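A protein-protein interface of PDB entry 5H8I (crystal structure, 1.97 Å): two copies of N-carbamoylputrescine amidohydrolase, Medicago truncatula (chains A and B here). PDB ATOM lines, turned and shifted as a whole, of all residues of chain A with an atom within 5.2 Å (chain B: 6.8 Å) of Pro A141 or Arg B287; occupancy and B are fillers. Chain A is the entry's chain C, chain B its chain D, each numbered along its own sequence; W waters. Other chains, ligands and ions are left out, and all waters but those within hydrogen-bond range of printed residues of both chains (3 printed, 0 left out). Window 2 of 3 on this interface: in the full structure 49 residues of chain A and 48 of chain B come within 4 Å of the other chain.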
ATOM      1  N   TYR A 106     -24.510  24.787  29.409  1.00  0.00           N
ATOM      2  CA  TYR A 106     -24.225  24.833  28.019  1.00  0.00           C
ATOM      3  C   TYR A 106     -22.764  24.575  27.733  1.00  0.00           C
ATOM      4  O   TYR A 106     -21.905  24.731  28.616  1.00  0.00           O
ATOM      5  CB  TYR A 106     -24.572  26.196  27.461  1.00  0.00           C
ATOM      6  CG  TYR A 106     -25.965  26.703  27.676  1.00  0.00           C
ATOM      7  CD1 TYR A 106     -27.021  26.358  26.797  1.00  0.00           C
ATOM      8  CD2 TYR A 106     -26.261  27.572  28.760  1.00  0.00           C
ATOM      9  CE1 TYR A 106     -28.282  26.862  27.002  1.00  0.00           C
ATOM     10  CE2 TYR A 106     -27.532  28.059  28.937  1.00  0.00           C
ATOM     11  CZ  TYR A 106     -28.515  27.702  28.063  1.00  0.00           C
ATOM     12  OH  TYR A 106     -29.735  28.202  28.263  1.00  0.00           O
ATOM     13  N   LYS A 124     -23.284  26.173  22.105  1.00  0.00           N
ATOM     14  CA  LYS A 124     -23.328  25.040  21.148  1.00  0.00           C
ATOM     15  C   LYS A 124     -24.780  24.617  20.848  1.00  0.00           C
ATOM     16  O   LYS A 124     -25.553  24.353  21.773  1.00  0.00           O
ATOM     17  CB  LYS A 124     -22.504  23.875  21.669  1.00  0.00           C
ATOM     18  CG  LYS A 124     -22.304  22.733  20.687  1.00  0.00           C
ATOM     19  CD  LYS A 124     -21.348  21.689  21.273  1.00  0.00           C
ATOM     20  CE  LYS A 124     -21.010  20.645  20.221  1.00  0.00           C
ATOM     21  NZ  LYS A 124     -20.048  19.721  20.790  1.00  0.00           N
ATOM     22  N   SER A 125     -25.116  24.567  19.548  1.00  0.00           N
ATOM     23  CA  SER A 125     -26.447  24.309  19.102  1.00  0.00           C
ATOM     24  C   SER A 125     -26.789  22.834  18.895  1.00  0.00           C
ATOM     25  O   SER A 125     -27.862  22.380  19.287  1.00  0.00           O
ATOM     26  CB  SER A 125     -26.710  25.054  17.794  1.00  0.00           C
ATOM     27  OG  SER A 125     -26.571  26.427  17.947  1.00  0.00           O
ATOM     28  N   HIS A 126     -25.877  22.105  18.274  1.00  0.00           N
ATOM     29  CA  HIS A 126     -26.080  20.708  17.914  1.00  0.00           C
ATOM     30  C   HIS A 126     -25.291  19.913  18.895  1.00  0.00           C
ATOM     31  O   HIS A 126     -24.075  20.070  18.958  1.00  0.00           O
ATOM     32  CB  HIS A 126     -25.553  20.458  16.502  1.00  0.00           C
ATOM     33  CG  HIS A 126     -26.145  21.341  15.460  1.00  0.00           C
ATOM     34  ND1 HIS A 126     -25.506  22.466  15.002  1.00  0.00           N
ATOM     35  CD2 HIS A 126     -27.314  21.266  14.779  1.00  0.00           C
ATOM     36  CE1 HIS A 126     -26.255  23.055  14.079  1.00  0.00           C
ATOM     37  NE2 HIS A 126     -27.358  22.346  13.923  1.00  0.00           N
ATOM     38  N   ILE A 127     -25.957  19.073  19.684  1.00  0.00           N
ATOM     39  CA  ILE A 127     -25.282  18.344  20.764  1.00  0.00           C
ATOM     40  C   ILE A 127     -25.157  16.860  20.416  1.00  0.00           C
ATOM     41  O   ILE A 127     -26.164  16.197  20.227  1.00  0.00           O
ATOM     42  CB  ILE A 127     -26.063  18.481  22.076  1.00  0.00           C
ATOM     43  CG1 ILE A 127     -26.445  19.949  22.328  1.00  0.00           C
ATOM     44  CG2 ILE A 127     -25.259  17.877  23.252  1.00  0.00           C
ATOM     45  CD1 ILE A 127     -25.261  20.914  22.440  1.00  0.00           C
ATOM     46  N   PHE A 139     -25.429  19.102  28.369  1.00  0.00           N
ATOM     47  CA  PHE A 139     -25.722  20.412  27.817  1.00  0.00           C
ATOM     48  C   PHE A 139     -27.148  20.595  27.272  1.00  0.00           C
ATOM     49  O   PHE A 139     -27.654  19.784  26.447  1.00  0.00           O
ATOM     50  CB  PHE A 139     -24.746  20.730  26.673  1.00  0.00           C
ATOM     51  CG  PHE A 139     -23.307  20.424  26.973  1.00  0.00           C
ATOM     52  CD1 PHE A 139     -22.647  21.040  28.030  1.00  0.00           C
ATOM     53  CD2 PHE A 139     -22.594  19.533  26.185  1.00  0.00           C
ATOM     54  CE1 PHE A 139     -21.340  20.743  28.289  1.00  0.00           C
ATOM     55  CE2 PHE A 139     -21.273  19.240  26.443  1.00  0.00           C
ATOM     56  CZ  PHE A 139     -20.635  19.843  27.498  1.00  0.00           C
ATOM     57  N   ASN A 140     -27.797  21.673  27.716  1.00  0.00           N
ATOM     58  CA  ASN A 140     -29.012  22.118  27.083  1.00  0.00           C
ATOM     59  C   ASN A 140     -28.586  22.430  25.668  1.00  0.00           C
ATOM     60  O   ASN A 140     -27.497  22.955  25.456  1.00  0.00           O
ATOM     61  CB  ASN A 140     -29.585  23.407  27.676  1.00  0.00           C
ATOM     62  CG  ASN A 140     -30.216  23.240  29.057  1.00  0.00           C
ATOM     63  OD1 ASN A 140     -29.554  23.044  30.050  1.00  0.00           O
ATOM     64  ND2 ASN A 140     -31.513  23.364  29.108  1.00  0.00           N
ATOM     65  N   PRO A 141     -29.428  22.121  24.675  1.00  0.00           N
ATOM     66  CA  PRO A 141     -29.100  22.591  23.326  1.00  0.00           C
ATOM     67  C   PRO A 141     -29.047  24.117  23.344  1.00  0.00           C
ATOM     68  O   PRO A 141     -29.863  24.726  23.986  1.00  0.00           O
ATOM     69  CB  PRO A 141     -30.261  22.081  22.491  1.00  0.00           C
ATOM     70  CG  PRO A 141     -30.742  20.881  23.247  1.00  0.00           C
ATOM     71  CD  PRO A 141     -30.663  21.323  24.681  1.00  0.00           C
ATOM     72  N   GLY A 142     -28.090  24.694  22.675  1.00  0.00           N
ATOM     73  CA  GLY A 142     -27.836  26.120  22.794  1.00  0.00           C
ATOM     74  C   GLY A 142     -28.999  26.965  22.291  1.00  0.00           C
ATOM     75  O   GLY A 142     -29.769  26.545  21.379  1.00  0.00           O
ATOM     76  N   ASP A 143     -29.126  28.147  22.880  1.00  0.00           N
ATOM     77  CA  ASP A 143     -30.200  29.015  22.581  1.00  0.00           C
ATOM     78  C   ASP A 143     -29.765  30.437  22.148  1.00  0.00           C
ATOM     79  O   ASP A 143     -30.610  31.326  22.065  1.00  0.00           O
ATOM     80  CB  ASP A 143     -31.144  29.087  23.784  1.00  0.00           C
ATOM     81  CG  ASP A 143     -30.407  29.445  25.123  1.00  0.00           C
ATOM     82  OD1 ASP A 143     -29.220  29.923  25.076  1.00  0.00           O
ATOM     83  OD2 ASP A 143     -31.016  29.227  26.194  1.00  0.00           O
ATOM     84  N   LEU A 297     -37.834  18.668  10.639  1.00  0.00           N
ATOM     85  CA  LEU A 297     -36.921  17.584  10.945  1.00  0.00           C
ATOM     86  C   LEU A 297     -37.223  16.363  10.024  1.00  0.00           C
ATOM     87  O   LEU A 297     -36.327  15.614   9.663  1.00  0.00           O
ATOM     88  CB  LEU A 297     -37.067  17.161  12.420  1.00  0.00           C
ATOM     89  CG  LEU A 297     -36.606  18.163  13.453  1.00  0.00           C
ATOM     90  CD1 LEU A 297     -37.059  17.719  14.846  1.00  0.00           C
ATOM     91  CD2 LEU A 297     -35.110  18.362  13.390  1.00  0.00           C
ATOM     92  N   VAL B 282     -26.728  13.045  12.784  1.00  0.00           N
ATOM     93  CA  VAL B 282     -26.921  14.418  12.344  1.00  0.00           C
ATOM     94  C   VAL B 282     -28.389  14.793  12.207  1.00  0.00           C
ATOM     95  O   VAL B 282     -28.776  15.890  12.621  1.00  0.00           O
ATOM     96  CB  VAL B 282     -26.122  14.784  11.104  1.00  0.00           C
ATOM     97  CG1 VAL B 282     -24.626  14.718  11.418  1.00  0.00           C
ATOM     98  CG2 VAL B 282     -26.460  13.881   9.907  1.00  0.00           C
ATOM     99  N   ARG B 284     -30.920  13.536  13.797  1.00  0.00           N
ATOM    100  CA  ARG B 284     -31.470  13.554  15.131  1.00  0.00           C
ATOM    101  C   ARG B 284     -31.174  14.919  15.834  1.00  0.00           C
ATOM    102  O   ARG B 284     -31.905  15.335  16.716  1.00  0.00           O
ATOM    103  CB  ARG B 284     -30.834  12.432  15.935  1.00  0.00           C
ATOM    104  CG  ARG B 284     -31.300  12.268  17.396  1.00  0.00           C
ATOM    105  CD  ARG B 284     -30.345  11.372  18.175  1.00  0.00           C
ATOM    106  NE  ARG B 284     -29.018  11.965  18.097  1.00  0.00           N
ATOM    107  CZ  ARG B 284     -27.876  11.285  18.227  1.00  0.00           C
ATOM    108  NH1 ARG B 284     -27.897   9.976  18.463  1.00  0.00           N
ATOM    109  NH2 ARG B 284     -26.706  11.917  18.112  1.00  0.00           N
ATOM    110  N   ASP B 285     -30.103  15.573  15.416  1.00  0.00           N
ATOM    111  CA  ASP B 285     -29.520  16.669  16.178  1.00  0.00           C
ATOM    112  C   ASP B 285     -29.732  18.041  15.545  1.00  0.00           C
ATOM    113  O   ASP B 285     -29.324  19.063  16.139  1.00  0.00           O
ATOM    114  CB  ASP B 285     -28.022  16.404  16.361  1.00  0.00           C
ATOM    115  CG  ASP B 285     -27.725  15.143  17.171  1.00  0.00           C
ATOM    116  OD1 ASP B 285     -28.623  14.667  17.934  1.00  0.00           O
ATOM    117  OD2 ASP B 285     -26.555  14.623  17.071  1.00  0.00           O
ATOM    118  N   ARG B 286     -30.368  18.070  14.346  1.00  0.00           N
ATOM    119  CA  ARG B 286     -30.628  19.312  13.643  1.00  0.00           C
ATOM    120  C   ARG B 286     -31.525  20.240  14.481  1.00  0.00           C
ATOM    121  O   ARG B 286     -32.350  19.796  15.305  1.00  0.00           O
ATOM    122  CB  ARG B 286     -31.258  19.054  12.265  1.00  0.00           C
ATOM    123  CG  ARG B 286     -30.303  18.435  11.281  1.00  0.00           C
ATOM    124  CD  ARG B 286     -30.856  18.214   9.892  1.00  0.00           C
ATOM    125  NE  ARG B 286     -31.231  19.467   9.214  1.00  0.00           N
ATOM    126  CZ  ARG B 286     -32.474  19.935   9.139  1.00  0.00           C
ATOM    127  NH1 ARG B 286     -33.486  19.256   9.697  1.00  0.00           N
ATOM    128  NH2 ARG B 286     -32.719  21.081   8.488  1.00  0.00           N
ATOM    129  N   ARG B 287     -31.336  21.533  14.249  1.00  0.00           N
ATOM    130  CA  ARG B 287     -31.972  22.583  14.990  1.00  0.00           C
ATOM    131  C   ARG B 287     -32.741  23.519  14.089  1.00  0.00           C
ATOM    132  O   ARG B 287     -32.380  24.692  13.942  1.00  0.00           O
ATOM    133  CB  ARG B 287     -30.921  23.392  15.770  1.00  0.00           C
ATOM    134  CG  ARG B 287     -30.195  22.609  16.859  1.00  0.00           C
ATOM    135  CD  ARG B 287     -31.109  22.236  17.997  1.00  0.00           C
ATOM    136  NE  ARG B 287     -31.842  23.383  18.543  1.00  0.00           N
ATOM    137  CZ  ARG B 287     -31.342  24.255  19.440  1.00  0.00           C
ATOM    138  NH1 ARG B 287     -30.099  24.118  19.889  1.00  0.00           N
ATOM    139  NH2 ARG B 287     -32.077  25.248  19.864  1.00  0.00           N
ATOM    140  N   PRO B 288     -33.832  23.043  13.493  1.00  0.00           N
ATOM    141  CA  PRO B 288     -34.586  23.923  12.636  1.00  0.00           C
ATOM    142  C   PRO B 288     -35.114  25.186  13.332  1.00  0.00           C
ATOM    143  O   PRO B 288     -35.328  26.240  12.663  1.00  0.00           O
ATOM    144  CB  PRO B 288     -35.718  22.995  12.095  1.00  0.00           C
ATOM    145  CG  PRO B 288     -35.801  21.846  13.020  1.00  0.00           C
ATOM    146  CD  PRO B 288     -34.396  21.678  13.521  1.00  0.00           C
ATOM    147  N   ASP B 289     -35.324  25.144  14.645  1.00  0.00           N
ATOM    148  CA  ASP B 289     -35.697  26.358  15.384  1.00  0.00           C
ATOM    149  C   ASP B 289     -34.659  27.511  15.283  1.00  0.00           C
ATOM    150  O   ASP B 289     -34.988  28.671  15.536  1.00  0.00           O
ATOM    151  CB  ASP B 289     -36.028  26.055  16.870  1.00  0.00           C
ATOM    152  CG  ASP B 289     -34.866  25.317  17.651  1.00  0.00           C
ATOM    153  OD1 ASP B 289     -34.052  24.550  17.030  1.00  0.00           O
ATOM    154  OD2 ASP B 289     -34.788  25.506  18.869  1.00  0.00           O
ATOM    155  N   LEU B 290     -33.412  27.177  14.921  1.00  0.00           N
ATOM    156  CA  LEU B 290     -32.336  28.158  14.794  1.00  0.00           C
ATOM    157  C   LEU B 290     -31.969  28.440  13.338  1.00  0.00           C
ATOM    158  O   LEU B 290     -30.978  29.151  13.062  1.00  0.00           O
ATOM    159  CB  LEU B 290     -31.096  27.633  15.540  1.00  0.00           C
ATOM    160  CG  LEU B 290     -31.224  27.324  17.023  1.00  0.00           C
ATOM    161  CD1 LEU B 290     -29.876  26.828  17.533  1.00  0.00           C
ATOM    162  CD2 LEU B 290     -31.732  28.522  17.810  1.00  0.00           C
ATOM    163  N   TYR B 291     -32.742  27.881  12.386  1.00  0.00           N
ATOM    164  CA  TYR B 291     -32.361  27.979  10.947  1.00  0.00           C
ATOM    165  C   TYR B 291     -33.171  29.036  10.182  1.00  0.00           C
ATOM    166  O   TYR B 291     -33.074  29.103   8.974  1.00  0.00           O
ATOM    167  CB  TYR B 291     -32.436  26.636  10.184  1.00  0.00           C
ATOM    168  CG  TYR B 291     -31.580  25.474  10.705  1.00  0.00           C
ATOM    169  CD1 TYR B 291     -30.434  25.685  11.472  1.00  0.00           C
ATOM    170  CD2 TYR B 291     -31.934  24.182  10.417  1.00  0.00           C
ATOM    171  CE1 TYR B 291     -29.680  24.629  11.945  1.00  0.00           C
ATOM    172  CE2 TYR B 291     -31.195  23.115  10.875  1.00  0.00           C
ATOM    173  CZ  TYR B 291     -30.072  23.335  11.644  1.00  0.00           C
ATOM    174  OH  TYR B 291     -29.340  22.277  12.110  1.00  0.00           O
ATOM    175  N   LYS B 292     -33.948  29.861  10.872  1.00  0.00           N
ATOM    176  CA  LYS B 292     -34.768  30.820  10.168  1.00  0.00           C
ATOM    177  C   LYS B 292     -33.921  31.801   9.335  1.00  0.00           C
ATOM    178  O   LYS B 292     -34.387  32.259   8.323  1.00  0.00           O
ATOM    179  CB  LYS B 292     -35.669  31.579  11.109  1.00  0.00           C
ATOM    180  CG  LYS B 292     -36.798  30.712  11.674  1.00  0.00           C
ATOM    181  CD  LYS B 292     -37.677  31.556  12.556  1.00  0.00           C
ATOM    182  CE  LYS B 292     -39.007  30.859  12.849  1.00  0.00           C
ATOM    183  NZ  LYS B 292     -38.749  29.762  13.798  1.00  0.00           N
HETATM  184  O   HOH W   1     -28.737  18.656  18.873  1.00  0.00           O
HETATM  185  O   HOH W   2     -33.660  16.404  10.649  1.00  0.00           O
HETATM  186  O   HOH W   3     -32.546  25.398  23.152  1.00  0.00           O
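Water W1 bridges the backbone carbonyl oxygen of Asp B285 (2.8 Å) and the backbone NH of Ile A127 (2.9 Å).
Water W3 lies within hydrogen-bond range of O of Pro A141 (2.9 Å), NH2 of Arg B287 (3.3 Å) and O of Gly A142 (3.5 Å).
Water W2 lies within hydrogen-bond range of O of Leu A297 and NH1 of Arg B286.
No position is printed for both chains.
Printed residues of chain A that touch a printed residue of chain B: Ser A125, His A126, Ile A127, Pro A141, Gly A142 and Leu A297.
Among the printed residues, no Asp or Glu carboxylate lies within 4 Å of a Lys or Arg side-chain nitrogen of the other chain.
Of chain A, only Ser A125, His A126, Pro A141 and Gly A142 come within 4 Å of Arg B287.
Printed residues of chain A within 4 Å of Tyr B291: His A126 (2.7 Å).
Of the printed residues of chain B, Ser A125 touches Arg B287 (2.9 Å) and Leu B290 (3.4 Å).
Of the printed residues of chain A, Arg B286 touches Leu A297.
Printed residues of chain B within 4 Å of Leu A297: Arg B286 and Pro B288.
Of the printed residues of chain B, His A126 touches Asp B285, Arg B287 and Tyr B291.
Asp A143 touches none of the printed residues of chain B.
Val B282 touches none of the printed residues of chain A.
The nearest residue of chain B that does not touch Pro A141 is Leu B290 (6.5 Å).
The nearest residue of chain A that does not touch Arg B287 is Lys A124 (4.9 Å).
The nearest printed residue of chain B that does not touch Ser A125 is Asp B285 (4.8 Å).
The guanidinium group (NH1) of Arg B287 lies within hydrogen-bond range of the backbone carbonyl oxygen (O) of Ser A125 (2.9 Å).
A ring nitrogen (NE2) of His A126 lies within hydrogen-bond range of the side-chain hydroxyl (OH) of Tyr B291, 2.7 Å away.
O of Gly A142 sits at hydrogen-bond distance from NH1 of Arg B287.
Leu B290 touches Ser A125 (CD1 to OG, 3.4 Å).
CD2 of His A126 touches O of Asp B285 (3.3 Å).
CD2 of His A126 touches CG of Arg B287, 3.8 Å away.
Asp B285 touches Ile A127 (OD2 to O, 3.5 Å).
Arg B287 touches Pro A141.
Gly A142 touches Leu B290.
Leu A297 touches Arg B286 (CD2 to O, 3.7 Å).
Leu A297 touches Pro B288 (CD2 to CD, 3.4 Å).
The backbone carbonyl oxygen (O) of Lys A124 sits at hydrogen-bond distance from the backbone NH (N) of Gly A142 (2.7 Å).
The guanidinium group (NE) of Arg B284 lies within salt-bridge range of the side-chain carboxylate (OD1) of Asp B285 (2.7 Å).
OD2 of Asp B289 is in salt-bridge range of NH2 of Arg B287.
The backbone NH (N) of Arg B287 lies within hydrogen-bond range of the side-chain hydroxyl (OH) of Tyr B291, at 3.0 Å.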
